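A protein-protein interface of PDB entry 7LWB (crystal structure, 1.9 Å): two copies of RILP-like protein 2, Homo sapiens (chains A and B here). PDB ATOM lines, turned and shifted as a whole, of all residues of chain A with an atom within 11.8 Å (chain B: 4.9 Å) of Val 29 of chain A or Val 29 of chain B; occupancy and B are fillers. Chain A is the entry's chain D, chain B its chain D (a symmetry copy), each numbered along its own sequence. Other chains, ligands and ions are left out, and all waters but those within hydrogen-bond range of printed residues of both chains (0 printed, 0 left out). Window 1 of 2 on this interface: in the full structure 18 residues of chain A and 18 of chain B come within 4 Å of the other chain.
OE1 of Glu 32 of chain A lies within salt-bridge range of NH1 of Arg 33 of chain B, at 2.9 Å.
NH1 of Arg 33 of chain A is in salt-bridge range of OE1 of Glu 32 of chain B (2.9 Å).
The guanidinium group of Arg 33 of chain A is in hydrogen-bond range of the side-chain amide oxygen of Asn 34 of chain A, at 2.8 Å.
Phe 21 of chain A touches Leu 26 of chain B (CG to CD2, 3.7 Å).
Val 29 of chain A touches Val 29 of chain B.
O of Arg 33 of chain B touches CD1 of Leu 36 of chain A, 3.7 Å away.
Printed residues of chain B within 4 Å of Val 29 of chain A: Val 29.
Of the printed residues of chain A, Val 29 of chain B touches Val 29 (3.5 Å).
Of the printed residues of chain A, Glu 32 of chain B touches Arg 33 (2.9 Å).
Of chain A, only Glu 32 and Leu 36 come within 4 Å of Arg 33 of chain B.
Of the printed residues of chain B, Leu 36 of chain A touches Arg 33.
Of the printed residues of chain B, Glu 32 of chain A touches Arg 33 (2.9 Å).
Of the printed residues of chain B, Arg 33 of chain A touches Glu 32 (2.9 Å).
Printed residues of chain B within 4 Å of Phe 21 of chain A: Leu 26.
The nearest printed residue of chain B that does not touch Glu 32 of chain A is Leu 30 of chain B (6.2 Å).
Hydrophobic or aromatic side chains of chain A that line the printed part of chain B: Phe 21, Val 29 and Leu 36.
Printed residues of chain B that touch a printed residue of chain A: Leu 26, Val 29, Glu 32 and Arg 33.
Among the printed residues, 5 pairs touch across the chains.
Among the printed residues, Asp or Glu carboxylates within 4 Å of a Lys or Arg side-chain nitrogen of the other chain: Glu 32 of chain A with Arg 33 of chain B (2.9 Å) and Arg 33 of chain A with Glu 32 of chain B (2.9 Å).
Val 29 of chain A touches its own counterpart, Val 29 of chain B.
Glu 32 of chain A touches Arg 33 of chain B, and with the chains exchanged Arg 33 of chain A touches Glu 32 of chain B.
Of the 5 pairs that touch across the chains among the printed residues, 3 have their exchanged pair printed and touching as well.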
ATOM      1  N   PHE A  21     -16.263  23.347  -8.340  1.00  0.00           N
ATOM      2  CA  PHE A  21     -17.116  22.385  -7.654  1.00  0.00           C
ATOM      3  C   PHE A  21     -18.572  22.592  -8.036  1.00  0.00           C
ATOM      4  O   PHE A  21     -19.000  23.707  -8.388  1.00  0.00           O
ATOM      5  CB  PHE A  21     -16.873  22.492  -6.154  1.00  0.00           C
ATOM      6  CG  PHE A  21     -15.423  22.362  -5.816  1.00  0.00           C
ATOM      7  CD1 PHE A  21     -14.822  21.115  -5.816  1.00  0.00           C
ATOM      8  CD2 PHE A  21     -14.646  23.494  -5.561  1.00  0.00           C
ATOM      9  CE1 PHE A  21     -13.461  20.971  -5.573  1.00  0.00           C
ATOM     10  CE2 PHE A  21     -13.287  23.364  -5.306  1.00  0.00           C
ATOM     11  CZ  PHE A  21     -12.695  22.085  -5.295  1.00  0.00           C
ATOM     12  N   THR A  22     -19.310  21.500  -7.977  1.00  0.00           N
ATOM     13  CA  THR A  22     -20.668  21.368  -8.455  1.00  0.00           C
ATOM     14  C   THR A  22     -21.673  21.913  -7.458  1.00  0.00           C
ATOM     15  O   THR A  22     -21.381  22.147  -6.269  1.00  0.00           O
ATOM     16  CB  THR A  22     -21.023  19.903  -8.691  1.00  0.00           C
ATOM     17  OG1 THR A  22     -20.857  19.209  -7.457  1.00  0.00           O
ATOM     18  CG2 THR A  22     -20.142  19.230  -9.825  1.00  0.00           C
ATOM     19  N   LEU A  23     -22.895  22.101  -7.958  1.00  0.00           N
ATOM     20  CA  LEU A  23     -23.977  22.463  -7.062  1.00  0.00           C
ATOM     21  C   LEU A  23     -24.106  21.427  -5.952  1.00  0.00           C
ATOM     22  O   LEU A  23     -24.134  21.762  -4.754  1.00  0.00           O
ATOM     23  CB  LEU A  23     -25.273  22.601  -7.861  1.00  0.00           C
ATOM     24  CG  LEU A  23     -26.555  22.891  -7.072  1.00  0.00           C
ATOM     25  CD1 LEU A  23     -26.378  24.109  -6.228  1.00  0.00           C
ATOM     26  CD2 LEU A  23     -27.692  23.082  -8.053  1.00  0.00           C
ATOM     27  N   GLN A  24     -24.159  20.160  -6.343  1.00  0.00           N
ATOM     28  CA  GLN A  24     -24.296  19.071  -5.390  1.00  0.00           C
ATOM     29  C   GLN A  24     -23.223  19.153  -4.311  1.00  0.00           C
ATOM     30  O   GLN A  24     -23.519  18.980  -3.110  1.00  0.00           O
ATOM     31  CB  GLN A  24     -24.245  17.728  -6.135  1.00  0.00           C
ATOM     32  CG  GLN A  24     -24.167  16.508  -5.181  1.00  0.00           C
ATOM     33  CD  GLN A  24     -22.742  15.959  -5.053  1.00  0.00           C
ATOM     34  OE1 GLN A  24     -22.300  15.579  -3.964  1.00  0.00           O
ATOM     35  NE2 GLN A  24     -22.019  15.897  -6.196  1.00  0.00           N
ATOM     36  N   GLU A  25     -21.972  19.404  -4.710  1.00  0.00           N
ATOM     37  CA  GLU A  25     -20.884  19.436  -3.742  1.00  0.00           C
ATOM     38  C   GLU A  25     -21.079  20.549  -2.729  1.00  0.00           C
ATOM     39  O   GLU A  25     -20.914  20.350  -1.514  1.00  0.00           O
ATOM     40  CB  GLU A  25     -19.547  19.586  -4.460  1.00  0.00           C
ATOM     41  CG  GLU A  25     -18.973  18.234  -4.840  1.00  0.00           C
ATOM     42  CD  GLU A  25     -17.981  18.293  -5.990  1.00  0.00           C
ATOM     43  OE1 GLU A  25     -17.936  19.346  -6.698  1.00  0.00           O
ATOM     44  OE2 GLU A  25     -17.280  17.270  -6.184  1.00  0.00           O
ATOM     45  N   LEU A  26     -21.408  21.753  -3.203  1.00  0.00           N
ATOM     46  CA  LEU A  26     -21.498  22.870  -2.261  1.00  0.00           C
ATOM     47  C   LEU A  26     -22.746  22.755  -1.407  1.00  0.00           C
ATOM     48  O   LEU A  26     -22.692  22.963  -0.180  1.00  0.00           O
ATOM     49  CB  LEU A  26     -21.494  24.226  -3.030  1.00  0.00           C
ATOM     50  CG  LEU A  26     -21.674  25.468  -2.146  1.00  0.00           C
ATOM     51  CD1 LEU A  26     -20.402  25.643  -1.363  1.00  0.00           C
ATOM     52  CD2 LEU A  26     -21.950  26.719  -2.982  1.00  0.00           C
ATOM     53  N   ARG A  27     -23.883  22.427  -2.030  1.00  0.00           N
ATOM     54  CA  ARG A  27     -25.134  22.377  -1.291  1.00  0.00           C
ATOM     55  C   ARG A  27     -25.075  21.316  -0.196  1.00  0.00           C
ATOM     56  O   ARG A  27     -25.552  21.559   0.922  1.00  0.00           O
ATOM     57  CB  ARG A  27     -26.314  22.140  -2.243  1.00  0.00           C
ATOM     58  CG  ARG A  27     -27.631  21.851  -1.501  1.00  0.00           C
ATOM     59  CD  ARG A  27     -28.768  21.538  -2.468  1.00  0.00           C
ATOM     60  NE  ARG A  27     -28.437  20.395  -3.331  1.00  0.00           N
ATOM     61  CZ  ARG A  27     -28.797  20.289  -4.628  1.00  0.00           C
ATOM     62  NH1 ARG A  27     -29.574  21.223  -5.223  1.00  0.00           N
ATOM     63  NH2 ARG A  27     -28.407  19.217  -5.339  1.00  0.00           N
ATOM     64  N   ASP A  28     -24.433  20.154  -0.474  1.00  0.00           N
ATOM     65  CA  ASP A  28     -24.273  19.119   0.559  1.00  0.00           C
ATOM     66  C   ASP A  28     -23.519  19.636   1.797  1.00  0.00           C
ATOM     67  O   ASP A  28     -23.957  19.432   2.951  1.00  0.00           O
ATOM     68  CB  ASP A  28     -23.539  17.878   0.001  1.00  0.00           C
ATOM     69  CG  ASP A  28     -24.412  17.019  -0.881  1.00  0.00           C
ATOM     70  OD1 ASP A  28     -25.630  17.276  -0.964  1.00  0.00           O
ATOM     71  OD2 ASP A  28     -23.859  16.070  -1.519  1.00  0.00           O
ATOM     72  N   VAL A  29     -22.339  20.222   1.589  1.00  0.00           N
ATOM     73  CA  VAL A  29     -21.584  20.770   2.716  1.00  0.00           C
ATOM     74  C   VAL A  29     -22.357  21.876   3.434  1.00  0.00           C
ATOM     75  O   VAL A  29     -22.307  21.991   4.671  1.00  0.00           O
ATOM     76  CB  VAL A  29     -20.218  21.285   2.257  1.00  0.00           C
ATOM     77  CG1 VAL A  29     -19.465  21.824   3.491  1.00  0.00           C
ATOM     78  CG2 VAL A  29     -19.471  20.225   1.526  1.00  0.00           C
ATOM     79  N   LEU A  30     -23.094  22.695   2.694  1.00  0.00           N
ATOM     80  CA  LEU A  30     -23.873  23.736   3.353  1.00  0.00           C
ATOM     81  C   LEU A  30     -24.942  23.132   4.240  1.00  0.00           C
ATOM     82  O   LEU A  30     -25.243  23.674   5.317  1.00  0.00           O
ATOM     83  CB  LEU A  30     -24.550  24.640   2.341  1.00  0.00           C
ATOM     84  CG  LEU A  30     -23.671  25.722   1.733  1.00  0.00           C
ATOM     85  CD1 LEU A  30     -24.279  26.158   0.412  1.00  0.00           C
ATOM     86  CD2 LEU A  30     -23.575  26.908   2.756  1.00  0.00           C
ATOM     87  N   GLN A  31     -25.609  22.098   3.741  1.00  0.00           N
ATOM     88  CA  GLN A  31     -26.707  21.521   4.485  1.00  0.00           C
ATOM     89  C   GLN A  31     -26.206  20.883   5.777  1.00  0.00           C
ATOM     90  O   GLN A  31     -26.879  20.958   6.802  1.00  0.00           O
ATOM     91  CB  GLN A  31     -27.454  20.506   3.626  1.00  0.00           C
ATOM     92  CG  GLN A  31     -28.386  21.148   2.635  1.00  0.00           C
ATOM     93  CD  GLN A  31     -28.988  20.126   1.725  1.00  0.00           C
ATOM     94  OE1 GLN A  31     -28.383  19.088   1.467  1.00  0.00           O
ATOM     95  NE2 GLN A  31     -30.198  20.379   1.261  1.00  0.00           N
ATOM     96  N   GLU A  32     -25.020  20.268   5.723  1.00  0.00           N
ATOM     97  CA  GLU A  32     -24.381  19.714   6.909  1.00  0.00           C
ATOM     98  C   GLU A  32     -23.963  20.831   7.863  1.00  0.00           C
ATOM     99  O   GLU A  32     -24.105  20.714   9.085  1.00  0.00           O
ATOM    100  CB  GLU A  32     -23.168  18.865   6.509  1.00  0.00           C
ATOM    101  CG  GLU A  32     -22.358  18.402   7.714  1.00  0.00           C
ATOM    102  CD  GLU A  32     -21.154  17.507   7.382  1.00  0.00           C
ATOM    103  OE1 GLU A  32     -20.656  17.563   6.216  1.00  0.00           O
ATOM    104  OE2 GLU A  32     -20.758  16.720   8.304  1.00  0.00           O
ATOM    105  N   ARG A  33     -23.421  21.913   7.315  1.00  0.00           N
ATOM    106  CA  ARG A  33     -23.081  23.077   8.133  1.00  0.00           C
ATOM    107  C   ARG A  33     -24.300  23.610   8.887  1.00  0.00           C
ATOM    108  O   ARG A  33     -24.213  23.997  10.063  1.00  0.00           O
ATOM    109  CB  ARG A  33     -22.465  24.157   7.230  1.00  0.00           C
ATOM    110  CG  ARG A  33     -21.838  25.322   7.986  1.00  0.00           C
ATOM    111  CD  ARG A  33     -22.852  26.374   8.366  1.00  0.00           C
ATOM    112  NE  ARG A  33     -23.890  26.707   7.379  1.00  0.00           N
ATOM    113  CZ  ARG A  33     -23.785  27.680   6.458  1.00  0.00           C
ATOM    114  NH1 ARG A  33     -22.655  28.394   6.308  1.00  0.00           N
ATOM    115  NH2 ARG A  33     -24.810  27.889   5.636  1.00  0.00           N
ATOM    116  N   ASN A  34     -25.449  23.644   8.225  1.00  0.00           N
ATOM    117  CA  ASN A  34     -26.655  24.108   8.896  1.00  0.00           C
ATOM    118  C   ASN A  34     -27.081  23.152   9.999  1.00  0.00           C
ATOM    119  O   ASN A  34     -27.524  23.584  11.081  1.00  0.00           O
ATOM    120  CB  ASN A  34     -27.777  24.230   7.889  1.00  0.00           C
ATOM    121  CG  ASN A  34     -27.565  25.371   6.931  1.00  0.00           C
ATOM    122  OD1 ASN A  34     -26.668  26.228   7.108  1.00  0.00           O
ATOM    123  ND2 ASN A  34     -28.418  25.402   5.908  1.00  0.00           N
ATOM    124  N   LYS A  35     -27.059  21.851   9.687  1.00  0.00           N
ATOM    125  CA  LYS A  35     -27.480  20.837  10.648  1.00  0.00           C
ATOM    126  C   LYS A  35     -26.611  20.884  11.893  1.00  0.00           C
ATOM    127  O   LYS A  35     -27.123  20.803  13.008  1.00  0.00           O
ATOM    128  CB  LYS A  35     -27.445  19.450  10.001  1.00  0.00           C
ATOM    129  CG  LYS A  35     -27.732  18.290  10.969  1.00  0.00           C
ATOM    130  CD  LYS A  35     -27.592  16.885  10.303  1.00  0.00           C
ATOM    131  CE  LYS A  35     -26.139  16.479  10.153  1.00  0.00           C
ATOM    132  NZ  LYS A  35     -25.552  16.144  11.475  1.00  0.00           N
ATOM    133  N   LEU A  36     -25.301  21.053  11.718  1.00  0.00           N
ATOM    134  CA  LEU A  36     -24.377  21.139  12.838  1.00  0.00           C
ATOM    135  C   LEU A  36     -24.621  22.394  13.677  1.00  0.00           C
ATOM    136  O   LEU A  36     -24.722  22.314  14.907  1.00  0.00           O
ATOM    137  CB  LEU A  36     -22.946  21.105  12.330  1.00  0.00           C
ATOM    138  CG  LEU A  36     -22.607  19.693  11.821  1.00  0.00           C
ATOM    139  CD1 LEU A  36     -21.230  19.708  11.205  1.00  0.00           C
ATOM    140  CD2 LEU A  36     -22.663  18.734  12.982  1.00  0.00           C
ATOM    141  N   LYS A  37     -24.740  23.557  13.021  1.00  0.00           N
ATOM    142  CA  LYS A  37     -24.979  24.786  13.747  1.00  0.00           C
ATOM    143  C   LYS A  37     -26.277  24.698  14.543  1.00  0.00           C
ATOM    144  O   LYS A  37     -26.331  25.091  15.710  1.00  0.00           O
ATOM    145  CB  LYS A  37     -25.011  25.966  12.770  1.00  0.00           C
ATOM    146  CG  LYS A  37     -24.875  27.290  13.442  1.00  0.00           C
ATOM    147  CD  LYS A  37     -24.563  28.423  12.411  1.00  0.00           C
ATOM    148  CE  LYS A  37     -25.326  29.665  12.719  1.00  0.00           C
ATOM    149  NZ  LYS A  37     -24.539  30.899  13.227  1.00  0.00           N
ATOM    150  N   SER A  38     -27.326  24.186  13.916  1.00  0.00           N
ATOM    151  CA  SER A  38     -28.598  23.966  14.581  1.00  0.00           C
ATOM    152  C   SER A  38     -28.440  23.073  15.825  1.00  0.00           C
ATOM    153  O   SER A  38     -28.936  23.410  16.909  1.00  0.00           O
ATOM    154  CB  SER A  38     -29.557  23.345  13.560  1.00  0.00           C
ATOM    155  OG  SER A  38     -30.872  23.248  14.072  1.00  0.00           O
ATOM    156  N   GLN A  39     -27.719  21.946  15.686  1.00  0.00           N
ATOM    157  CA  GLN A  39     -27.545  21.022  16.813  1.00  0.00           C
ATOM    158  C   GLN A  39     -26.704  21.666  17.904  1.00  0.00           C
ATOM    159  O   GLN A  39     -26.979  21.485  19.094  1.00  0.00           O
ATOM    160  CB  GLN A  39     -26.894  19.701  16.348  1.00  0.00           C
ATOM    161  CG  GLN A  39     -27.742  18.874  15.385  1.00  0.00           C
ATOM    162  CD  GLN A  39     -26.960  17.789  14.571  1.00  0.00           C
ATOM    163  OE1 GLN A  39     -27.571  16.846  14.044  1.00  0.00           O
ATOM    164  NE2 GLN A  39     -25.635  17.936  14.456  1.00  0.00           N
ATOM    165  N   GLU B  25     -14.780  29.330  -2.162  1.00  0.00           N
ATOM    166  CA  GLU B  25     -16.147  29.133  -1.700  1.00  0.00           C
ATOM    167  C   GLU B  25     -16.296  27.818  -0.958  1.00  0.00           C
ATOM    168  O   GLU B  25     -16.908  27.753   0.121  1.00  0.00           O
ATOM    169  CB  GLU B  25     -17.114  29.202  -2.877  1.00  0.00           C
ATOM    170  CG  GLU B  25     -17.562  30.627  -3.138  1.00  0.00           C
ATOM    171  CD  GLU B  25     -18.053  30.864  -4.557  1.00  0.00           C
ATOM    172  OE1 GLU B  25     -17.787  29.995  -5.443  1.00  0.00           O
ATOM    173  OE2 GLU B  25     -18.675  31.934  -4.769  1.00  0.00           O
ATOM    174  N   LEU B  26     -15.763  26.734  -1.526  1.00  0.00           N
ATOM    175  CA  LEU B  26     -15.981  25.436  -0.888  1.00  0.00           C
ATOM    176  C   LEU B  26     -15.147  25.307   0.372  1.00  0.00           C
ATOM    177  O   LEU B  26     -15.645  24.838   1.413  1.00  0.00           O
ATOM    178  CB  LEU B  26     -15.642  24.282  -1.880  1.00  0.00           C
ATOM    179  CG  LEU B  26     -15.750  22.870  -1.288  1.00  0.00           C
ATOM    180  CD1 LEU B  26     -17.214  22.583  -1.092  1.00  0.00           C
ATOM    181  CD2 LEU B  26     -15.130  21.822  -2.213  1.00  0.00           C
ATOM    182  N   ARG B  27     -13.875  25.714   0.304  1.00  0.00           N
ATOM    183  CA  ARG B  27     -12.991  25.548   1.448  1.00  0.00           C
ATOM    184  C   ARG B  27     -13.498  26.345   2.645  1.00  0.00           C
ATOM    185  O   ARG B  27     -13.462  25.843   3.778  1.00  0.00           O
ATOM    186  CB  ARG B  27     -11.553  25.936   1.079  1.00  0.00           C
ATOM    187  CG  ARG B  27     -10.620  26.000   2.301  1.00  0.00           C
ATOM    188  CD  ARG B  27      -9.220  26.469   1.919  1.00  0.00           C
ATOM    189  NE  ARG B  27      -9.255  27.785   1.268  1.00  0.00           N
ATOM    190  CZ  ARG B  27      -8.444  28.157   0.256  1.00  0.00           C
ATOM    191  NH1 ARG B  27      -7.462  27.344  -0.197  1.00  0.00           N
ATOM    192  NH2 ARG B  27      -8.587  29.375  -0.297  1.00  0.00           N
ATOM    193  N   ASP B  28     -14.040  27.567   2.410  1.00  0.00           N
ATOM    194  CA  ASP B  28     -14.617  28.355   3.509  1.00  0.00           C
ATOM    195  C   ASP B  28     -15.754  27.613   4.233  1.00  0.00           C
ATOM    196  O   ASP B  28     -15.786  27.540   5.482  1.00  0.00           O
ATOM    197  CB  ASP B  28     -15.143  29.719   3.005  1.00  0.00           C
ATOM    198  CG  ASP B  28     -14.043  30.712   2.721  1.00  0.00           C
ATOM    199  OD1 ASP B  28     -12.871  30.428   3.044  1.00  0.00           O
ATOM    200  OD2 ASP B  28     -14.359  31.800   2.148  1.00  0.00           O
ATOM    201  N   VAL B  29     -16.746  27.138   3.478  1.00  0.00           N
ATOM    202  CA  VAL B  29     -17.842  26.389   4.094  1.00  0.00           C
ATOM    203  C   VAL B  29     -17.345  25.121   4.787  1.00  0.00           C
ATOM    204  O   VAL B  29     -17.845  24.740   5.859  1.00  0.00           O
ATOM    205  CB  VAL B  29     -18.915  26.046   3.059  1.00  0.00           C
ATOM    206  CG1 VAL B  29     -20.050  25.283   3.775  1.00  0.00           C
ATOM    207  CG2 VAL B  29     -19.383  27.271   2.354  1.00  0.00           C
ATOM    208  N   LEU B  30     -16.351  24.453   4.214  1.00  0.00           N
ATOM    209  CA  LEU B  30     -15.829  23.260   4.870  1.00  0.00           C
ATOM    210  C   LEU B  30     -15.193  23.609   6.200  1.00  0.00           C
ATOM    211  O   LEU B  30     -15.291  22.832   7.165  1.00  0.00           O
ATOM    212  CB  LEU B  30     -14.786  22.572   4.011  1.00  0.00           C
ATOM    213  CG  LEU B  30     -15.329  21.688   2.899  1.00  0.00           C
ATOM    214  CD1 LEU B  30     -14.255  21.526   1.838  1.00  0.00           C
ATOM    215  CD2 LEU B  30     -15.748  20.311   3.526  1.00  0.00           C
ATOM    216  N   GLN B  31     -14.433  24.698   6.225  1.00  0.00           N
ATOM    217  CA  GLN B  31     -13.716  25.050   7.430  1.00  0.00           C
ATOM    218  C   GLN B  31     -14.689  25.411   8.549  1.00  0.00           C
ATOM    219  O   GLN B  31     -14.442  25.084   9.708  1.00  0.00           O
ATOM    220  CB  GLN B  31     -12.748  26.196   7.155  1.00  0.00           C
ATOM    221  CG  GLN B  31     -11.488  25.748   6.467  1.00  0.00           C
ATOM    222  CD  GLN B  31     -10.635  26.917   6.094  1.00  0.00           C
ATOM    223  OE1 GLN B  31     -11.145  28.011   5.863  1.00  0.00           O
ATOM    224  NE2 GLN B  31      -9.330  26.721   6.070  1.00  0.00           N
ATOM    225  N   GLU B  32     -15.795  26.072   8.194  1.00  0.00           N
ATOM    226  CA  GLU B  32     -16.852  26.381   9.148  1.00  0.00           C
ATOM    227  C   GLU B  32     -17.547  25.101   9.608  1.00  0.00           C
ATOM    228  O   GLU B  32     -17.873  24.941  10.789  1.00  0.00           O
ATOM    229  CB  GLU B  32     -17.865  27.348   8.522  1.00  0.00           C
ATOM    230  CG  GLU B  32     -19.084  27.570   9.410  1.00  0.00           C
ATOM    231  CD  GLU B  32     -20.115  28.567   8.858  1.00  0.00           C
ATOM    232  OE1 GLU B  32     -20.140  28.788   7.609  1.00  0.00           O
ATOM    233  OE2 GLU B  32     -20.859  29.149   9.715  1.00  0.00           O
ATOM    234  N   ARG B  33     -17.799  24.189   8.676  1.00  0.00           N
ATOM    235  CA  ARG B  33     -18.369  22.890   9.032  1.00  0.00           C
ATOM    236  C   ARG B  33     -17.496  22.154  10.049  1.00  0.00           C
ATOM    237  O   ARG B  33     -17.997  21.522  10.993  1.00  0.00           O
ATOM    238  CB  ARG B  33     -18.558  22.061   7.752  1.00  0.00           C
ATOM    239  CG  ARG B  33     -19.371  20.787   7.946  1.00  0.00           C
ATOM    240  CD  ARG B  33     -18.526  19.635   8.436  1.00  0.00           C
ATOM    241  NE  ARG B  33     -17.183  19.482   7.857  1.00  0.00           N
ATOM    242  CZ  ARG B  33     -16.896  18.739   6.775  1.00  0.00           C
ATOM    243  NH1 ARG B  33     -17.857  18.125   6.063  1.00  0.00           N
ATOM    244  NH2 ARG B  33     -15.631  18.672   6.368  1.00  0.00           N
